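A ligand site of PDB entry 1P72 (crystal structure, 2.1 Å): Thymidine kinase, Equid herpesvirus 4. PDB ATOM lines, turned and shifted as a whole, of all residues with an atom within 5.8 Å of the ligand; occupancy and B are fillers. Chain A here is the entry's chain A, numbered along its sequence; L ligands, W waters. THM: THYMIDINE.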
ATOM      1  N   TYR A  16      22.437 -12.519 -14.829  1.00  0.00           N
ATOM      2  CA  TYR A  16      22.851 -11.118 -14.948  1.00  0.00           C
ATOM      3  C   TYR A  16      24.327 -10.905 -14.625  1.00  0.00           C
ATOM      4  O   TYR A  16      24.880 -11.555 -13.736  1.00  0.00           O
ATOM      5  CB  TYR A  16      21.973 -10.212 -14.098  1.00  0.00           C
ATOM      6  CG  TYR A  16      22.070 -10.421 -12.608  1.00  0.00           C
ATOM      7  CD1 TYR A  16      22.913  -9.617 -11.814  1.00  0.00           C
ATOM      8  CD2 TYR A  16      21.285 -11.386 -11.963  1.00  0.00           C
ATOM      9  CE1 TYR A  16      22.979  -9.806 -10.404  1.00  0.00           C
ATOM     10  CE2 TYR A  16      21.340 -11.570 -10.584  1.00  0.00           C
ATOM     11  CZ  TYR A  16      22.170 -10.784  -9.810  1.00  0.00           C
ATOM     12  OH  TYR A  16      22.212 -11.007  -8.442  1.00  0.00           O
ATOM     13  N   GLU A  42      16.319  -5.691 -22.513  1.00  0.00           N
ATOM     14  CA  GLU A  42      15.572  -5.890 -21.278  1.00  0.00           C
ATOM     15  C   GLU A  42      14.528  -4.775 -21.119  1.00  0.00           C
ATOM     16  O   GLU A  42      14.787  -3.617 -21.436  1.00  0.00           O
ATOM     17  CB  GLU A  42      16.524  -5.925 -20.063  1.00  0.00           C
ATOM     18  CG  GLU A  42      17.051  -7.329 -19.772  1.00  0.00           C
ATOM     19  CD  GLU A  42      17.876  -7.399 -18.510  1.00  0.00           C
ATOM     20  OE1 GLU A  42      18.458  -6.355 -18.097  1.00  0.00           O
ATOM     21  OE2 GLU A  42      17.916  -8.473 -17.879  1.00  0.00           O
ATOM     22  N   MET A  44      13.566  -2.560 -19.175  1.00  0.00           N
ATOM     23  CA  MET A  44      14.018  -1.775 -18.029  1.00  0.00           C
ATOM     24  C   MET A  44      13.006  -0.741 -17.560  1.00  0.00           C
ATOM     25  O   MET A  44      12.616  -0.753 -16.392  1.00  0.00           O
ATOM     26  CB  MET A  44      15.368  -1.104 -18.371  1.00  0.00           C
ATOM     27  CG  MET A  44      16.389  -0.986 -17.214  1.00  0.00           C
ATOM     28  SD  MET A  44      16.332  -2.145 -15.837  1.00  0.00           S
ATOM     29  CE  MET A  44      17.485  -3.372 -16.386  1.00  0.00           C
ATOM     30  N   TRP A  47       9.981  -2.249 -15.904  1.00  0.00           N
ATOM     31  CA  TRP A  47      10.322  -2.656 -14.543  1.00  0.00           C
ATOM     32  C   TRP A  47      10.484  -1.497 -13.567  1.00  0.00           C
ATOM     33  O   TRP A  47      10.081  -1.600 -12.397  1.00  0.00           O
ATOM     34  CB  TRP A  47      11.616  -3.456 -14.583  1.00  0.00           C
ATOM     35  CG  TRP A  47      11.518  -4.820 -15.213  1.00  0.00           C
ATOM     36  CD1 TRP A  47      10.401  -5.560 -15.390  1.00  0.00           C
ATOM     37  CD2 TRP A  47      12.607  -5.588 -15.718  1.00  0.00           C
ATOM     38  NE1 TRP A  47      10.724  -6.758 -15.984  1.00  0.00           N
ATOM     39  CE2 TRP A  47      12.073  -6.792 -16.195  1.00  0.00           C
ATOM     40  CE3 TRP A  47      13.991  -5.371 -15.838  1.00  0.00           C
ATOM     41  CZ2 TRP A  47      12.862  -7.794 -16.762  1.00  0.00           C
ATOM     42  CZ3 TRP A  47      14.782  -6.359 -16.404  1.00  0.00           C
ATOM     43  CH2 TRP A  47      14.218  -7.553 -16.861  1.00  0.00           C
ATOM     44  N   ILE A  56      12.825  -4.091  -9.454  1.00  0.00           N
ATOM     45  CA  ILE A  56      14.186  -4.518  -9.171  1.00  0.00           C
ATOM     46  C   ILE A  56      14.545  -4.047  -7.766  1.00  0.00           C
ATOM     47  O   ILE A  56      14.966  -4.851  -6.929  1.00  0.00           O
ATOM     48  CB  ILE A  56      15.182  -4.002 -10.241  1.00  0.00           C
ATOM     49  CG1 ILE A  56      15.116  -4.911 -11.480  1.00  0.00           C
ATOM     50  CG2 ILE A  56      16.629  -3.996  -9.681  1.00  0.00           C
ATOM     51  CD1 ILE A  56      15.593  -4.290 -12.761  1.00  0.00           C
ATOM     52  N   ILE A  59      12.169  -5.990  -5.218  1.00  0.00           N
ATOM     53  CA  ILE A  59      12.499  -7.381  -4.882  1.00  0.00           C
ATOM     54  C   ILE A  59      13.715  -7.478  -3.969  1.00  0.00           C
ATOM     55  O   ILE A  59      13.695  -8.253  -3.007  1.00  0.00           O
ATOM     56  CB  ILE A  59      12.620  -8.334  -6.135  1.00  0.00           C
ATOM     57  CG1 ILE A  59      12.629  -9.808  -5.682  1.00  0.00           C
ATOM     58  CG2 ILE A  59      13.864  -8.025  -6.975  1.00  0.00           C
ATOM     59  CD1 ILE A  59      12.137 -10.838  -6.707  1.00  0.00           C
ATOM     60  N   TYR A  60      14.756  -6.693  -4.240  1.00  0.00           N
ATOM     61  CA  TYR A  60      15.935  -6.672  -3.359  1.00  0.00           C
ATOM     62  C   TYR A  60      15.630  -6.005  -1.994  1.00  0.00           C
ATOM     63  O   TYR A  60      16.137  -6.453  -0.973  1.00  0.00           O
ATOM     64  CB  TYR A  60      17.168  -6.061  -4.048  1.00  0.00           C
ATOM     65  CG  TYR A  60      17.704  -6.903  -5.201  1.00  0.00           C
ATOM     66  CD1 TYR A  60      17.367  -6.608  -6.524  1.00  0.00           C
ATOM     67  CD2 TYR A  60      18.549  -7.999  -4.963  1.00  0.00           C
ATOM     68  CE1 TYR A  60      17.859  -7.381  -7.585  1.00  0.00           C
ATOM     69  CE2 TYR A  60      19.042  -8.780  -6.012  1.00  0.00           C
ATOM     70  CZ  TYR A  60      18.693  -8.455  -7.329  1.00  0.00           C
ATOM     71  OH  TYR A  60      19.171  -9.220  -8.374  1.00  0.00           O
ATOM     72  N   GLN A  84       8.448 -11.020  -8.616  1.00  0.00           N
ATOM     73  CA  GLN A  84       8.869 -11.933  -9.671  1.00  0.00           C
ATOM     74  C   GLN A  84       7.808 -12.024 -10.749  1.00  0.00           C
ATOM     75  O   GLN A  84       8.127 -12.209 -11.927  1.00  0.00           O
ATOM     76  CB  GLN A  84       9.136 -13.327  -9.081  1.00  0.00           C
ATOM     77  CG  GLN A  84      10.242 -14.208  -9.692  1.00  0.00           C
ATOM     78  CD  GLN A  84      11.249 -13.491 -10.574  1.00  0.00           C
ATOM     79  OE1 GLN A  84      12.230 -12.944 -10.076  1.00  0.00           O
ATOM     80  NE2 GLN A  84      10.997 -13.491 -11.888  1.00  0.00           N
ATOM     81  N   PHE A  87       8.217  -8.979 -13.056  1.00  0.00           N
ATOM     82  CA  PHE A  87       9.316  -9.133 -14.004  1.00  0.00           C
ATOM     83  C   PHE A  87       8.830  -9.736 -15.329  1.00  0.00           C
ATOM     84  O   PHE A  87       9.277  -9.335 -16.391  1.00  0.00           O
ATOM     85  CB  PHE A  87      10.429 -10.012 -13.429  1.00  0.00           C
ATOM     86  CG  PHE A  87      11.388  -9.280 -12.539  1.00  0.00           C
ATOM     87  CD1 PHE A  87      11.305  -9.407 -11.148  1.00  0.00           C
ATOM     88  CD2 PHE A  87      12.391  -8.484 -13.074  1.00  0.00           C
ATOM     89  CE1 PHE A  87      12.189  -8.724 -10.297  1.00  0.00           C
ATOM     90  CE2 PHE A  87      13.295  -7.801 -12.243  1.00  0.00           C
ATOM     91  CZ  PHE A  87      13.184  -7.904 -10.832  1.00  0.00           C
ATOM     92  N   THR A  88       7.896 -10.691 -15.241  1.00  0.00           N
ATOM     93  CA  THR A  88       7.516 -11.471 -16.416  1.00  0.00           C
ATOM     94  C   THR A  88       6.655 -10.690 -17.392  1.00  0.00           C
ATOM     95  O   THR A  88       6.691 -10.973 -18.582  1.00  0.00           O
ATOM     96  CB  THR A  88       6.790 -12.788 -16.070  1.00  0.00           C
ATOM     97  OG1 THR A  88       5.498 -12.503 -15.531  1.00  0.00           O
ATOM     98  CG2 THR A  88       7.499 -13.515 -14.968  1.00  0.00           C
ATOM     99  N   TYR A  91       7.784  -9.257 -20.796  1.00  0.00           N
ATOM    100  CA  TYR A  91       8.210 -10.390 -21.609  1.00  0.00           C
ATOM    101  C   TYR A  91       7.004 -11.089 -22.238  1.00  0.00           C
ATOM    102  O   TYR A  91       7.051 -11.425 -23.424  1.00  0.00           O
ATOM    103  CB  TYR A  91       9.044 -11.375 -20.777  1.00  0.00           C
ATOM    104  CG  TYR A  91      10.466 -10.912 -20.695  1.00  0.00           C
ATOM    105  CD1 TYR A  91      11.298 -11.006 -21.805  1.00  0.00           C
ATOM    106  CD2 TYR A  91      10.963 -10.336 -19.535  1.00  0.00           C
ATOM    107  CE1 TYR A  91      12.598 -10.571 -21.751  1.00  0.00           C
ATOM    108  CE2 TYR A  91      12.278  -9.882 -19.477  1.00  0.00           C
ATOM    109  CZ  TYR A  91      13.086 -10.007 -20.599  1.00  0.00           C
ATOM    110  OH  TYR A  91      14.391  -9.573 -20.609  1.00  0.00           O
ATOM    111  N   ARG A 121      16.926 -12.075 -23.235  1.00  0.00           N
ATOM    112  CA  ARG A 121      16.145 -13.054 -22.467  1.00  0.00           C
ATOM    113  C   ARG A 121      14.910 -13.588 -23.181  1.00  0.00           C
ATOM    114  O   ARG A 121      14.275 -12.888 -23.944  1.00  0.00           O
ATOM    115  CB  ARG A 121      15.732 -12.524 -21.072  1.00  0.00           C
ATOM    116  CG  ARG A 121      16.888 -11.930 -20.260  1.00  0.00           C
ATOM    117  CD  ARG A 121      16.505 -11.547 -18.819  1.00  0.00           C
ATOM    118  NE  ARG A 121      17.689 -11.178 -18.039  1.00  0.00           N
ATOM    119  CZ  ARG A 121      18.510 -12.053 -17.470  1.00  0.00           C
ATOM    120  NH1 ARG A 121      18.338 -13.353 -17.643  1.00  0.00           N
ATOM    121  NH2 ARG A 121      19.551 -11.631 -16.761  1.00  0.00           N
ATOM    122  N   ALA A 125      13.272 -17.026 -18.442  1.00  0.00           N
ATOM    123  CA  ALA A 125      14.078 -16.372 -17.401  1.00  0.00           C
ATOM    124  C   ALA A 125      13.229 -15.963 -16.175  1.00  0.00           C
ATOM    125  O   ALA A 125      13.553 -16.316 -15.029  1.00  0.00           O
ATOM    126  CB  ALA A 125      14.770 -15.123 -17.992  1.00  0.00           C
ATOM    127  N   SER A 126      12.137 -15.243 -16.437  1.00  0.00           N
ATOM    128  CA  SER A 126      11.343 -14.592 -15.406  1.00  0.00           C
ATOM    129  C   SER A 126      10.247 -15.528 -14.914  1.00  0.00           C
ATOM    130  O   SER A 126       9.752 -15.394 -13.805  1.00  0.00           O
ATOM    131  CB  SER A 126      10.804 -13.237 -15.902  1.00  0.00           C
ATOM    132  OG  SER A 126       9.933 -13.382 -17.030  1.00  0.00           O
ATOM    133  N   THR A 127       9.880 -16.514 -15.722  1.00  0.00           N
ATOM    134  CA  THR A 127       8.809 -17.405 -15.287  1.00  0.00           C
ATOM    135  C   THR A 127       9.320 -18.668 -14.665  1.00  0.00           C
ATOM    136  O   THR A 127       8.566 -19.344 -13.945  1.00  0.00           O
ATOM    137  CB  THR A 127       7.852 -17.765 -16.429  1.00  0.00           C
ATOM    138  OG1 THR A 127       8.571 -18.369 -17.516  1.00  0.00           O
ATOM    139  CG2 THR A 127       7.199 -16.499 -16.992  1.00  0.00           C
ATOM    140  N   PHE A 130      14.555 -17.584 -12.655  1.00  0.00           N
ATOM    141  CA  PHE A 130      14.741 -16.729 -11.494  1.00  0.00           C
ATOM    142  C   PHE A 130      13.830 -17.166 -10.345  1.00  0.00           C
ATOM    143  O   PHE A 130      14.289 -17.172  -9.215  1.00  0.00           O
ATOM    144  CB  PHE A 130      14.557 -15.252 -11.840  1.00  0.00           C
ATOM    145  CG  PHE A 130      15.816 -14.590 -12.368  1.00  0.00           C
ATOM    146  CD1 PHE A 130      16.207 -14.763 -13.703  1.00  0.00           C
ATOM    147  CD2 PHE A 130      16.590 -13.756 -11.553  1.00  0.00           C
ATOM    148  CE1 PHE A 130      17.359 -14.137 -14.204  1.00  0.00           C
ATOM    149  CE2 PHE A 130      17.725 -13.128 -12.050  1.00  0.00           C
ATOM    150  CZ  PHE A 130      18.118 -13.322 -13.392  1.00  0.00           C
ATOM    151  N   PRO A 131      12.549 -17.494 -10.622  1.00  0.00           N
ATOM    152  CA  PRO A 131      11.699 -18.129  -9.603  1.00  0.00           C
ATOM    153  C   PRO A 131      12.314 -19.405  -9.018  1.00  0.00           C
ATOM    154  O   PRO A 131      12.250 -19.582  -7.792  1.00  0.00           O
ATOM    155  CB  PRO A 131      10.422 -18.499 -10.375  1.00  0.00           C
ATOM    156  CG  PRO A 131      10.349 -17.490 -11.428  1.00  0.00           C
ATOM    157  CD  PRO A 131      11.791 -17.263 -11.866  1.00  0.00           C
ATOM    158  N   ARG A 134      15.061 -18.487  -6.588  1.00  0.00           N
ATOM    159  CA  ARG A 134      14.476 -17.927  -5.359  1.00  0.00           C
ATOM    160  C   ARG A 134      13.857 -19.012  -4.509  1.00  0.00           C
ATOM    161  O   ARG A 134      13.988 -18.990  -3.283  1.00  0.00           O
ATOM    162  CB  ARG A 134      13.423 -16.847  -5.680  1.00  0.00           C
ATOM    163  CG  ARG A 134      13.979 -15.567  -6.297  1.00  0.00           C
ATOM    164  CD  ARG A 134      14.691 -14.698  -5.307  1.00  0.00           C
ATOM    165  NE  ARG A 134      15.253 -13.478  -5.845  1.00  0.00           N
ATOM    166  CZ  ARG A 134      16.152 -12.746  -5.200  1.00  0.00           C
ATOM    167  NH1 ARG A 134      16.569 -13.148  -4.002  1.00  0.00           N
ATOM    168  NH2 ARG A 134      16.636 -11.630  -5.730  1.00  0.00           N
HETATM  169  O5' THM L   1      18.166  -8.452 -14.926  1.00  0.00           O
HETATM  170  C5' THM L   1      18.088  -7.175 -14.285  1.00  0.00           C
HETATM  171  C4' THM L   1      17.991  -7.336 -12.759  1.00  0.00           C
HETATM  172  O4' THM L   1      16.746  -7.949 -12.436  1.00  0.00           O
HETATM  173  C3' THM L   1      19.069  -8.216 -12.119  1.00  0.00           C
HETATM  174  O3' THM L   1      19.431  -7.637 -10.863  1.00  0.00           O
HETATM  175  C2' THM L   1      18.383  -9.565 -11.881  1.00  0.00           C
HETATM  176  C1' THM L   1      16.922  -9.187 -11.755  1.00  0.00           C
HETATM  177  N1  THM L   1      15.920 -10.098 -12.315  1.00  0.00           N
HETATM  178  C2  THM L   1      15.035 -10.744 -11.408  1.00  0.00           C
HETATM  179  O2  THM L   1      15.156 -10.608 -10.156  1.00  0.00           O
HETATM  180  N3  THM L   1      14.079 -11.544 -11.868  1.00  0.00           N
HETATM  181  C4  THM L   1      13.920 -11.732 -13.183  1.00  0.00           C
HETATM  182  O4  THM L   1      13.007 -12.483 -13.557  1.00  0.00           O
HETATM  183  C5  THM L   1      14.816 -11.072 -14.169  1.00  0.00           C
HETATM  184  C5M THM L   1      14.676 -11.271 -15.681  1.00  0.00           C
HETATM  185  C6  THM L   1      15.803 -10.239 -13.660  1.00  0.00           C
HETATM  186  O   HOH W   1      14.379 -13.027  -8.382  1.00  0.00           O
HETATM  187  O   HOH W   2      20.401  -6.549 -16.469  1.00  0.00           O
HETATM  188  O   HOH W   3      17.343 -11.635  -8.784  1.00  0.00           O
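The side-chain amide nitrogen (NE2) of Gln 84 sits at hydrogen-bond distance from an oxygen (O4) of the ligand (2.8 Å).
OH of Tyr 60 lies within hydrogen-bond range of O3' of the ligand (3.0 Å).
O5' of the ligand sits at hydrogen-bond distance from OE2 of Glu 42 (3.0 Å).
O of Ser 126 lies within hydrogen-bond range of NE2 of Gln 84 (3.0 Å).
OE2 of Glu 42 lies within salt-bridge range of NE of Arg 121 (2.7 Å).
N of Phe 130 is in hydrogen-bond range of O of Ala 125, 2.9 Å away.
NE1 of Trp 47 lies within hydrogen-bond range of O of Phe 87, 3.0 Å away.
CD2 of Tyr 16 touches C2' of the ligand, 3.4 Å away.
CH2 of Trp 47 touches C5M of the ligand (3.9 Å).
Ile 56 touches the ligand (CG1 to O4', 3.6 Å).
Phe 87 touches the ligand.
CD of Arg 121 touches C5M of the ligand, 3.6 Å away.
Ser 126 touches the ligand.
CD2 of Phe 130 touches N3 of the ligand, 3.4 Å away.
Hydrophobic or aromatic side chains within 4 Å of the ligand: Tyr 16, Trp 47, Ile 56, Tyr 60, Phe 87 and Phe 130.
Of the 18 residues printed, 10 come within 4 Å of the ligand.
The nearest printed residue that does not touch the ligand is Ala 125 (4.1 Å).
Water W3 lies within hydrogen-bond range of an oxygen (O2) of the ligand (2.8 Å), the side-chain hydroxyl of Tyr 60 (3.1 Å) and the guanidinium group of Arg 134 (3.1 Å).
Water W1 lies within hydrogen-bond range of NE of Arg 134 (2.7 Å), OE1 of Gln 84 (2.7 Å) and O2 of the ligand (3.1 Å).
Water W2 bridges OE1 of Glu 42 and O5' of the ligand.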
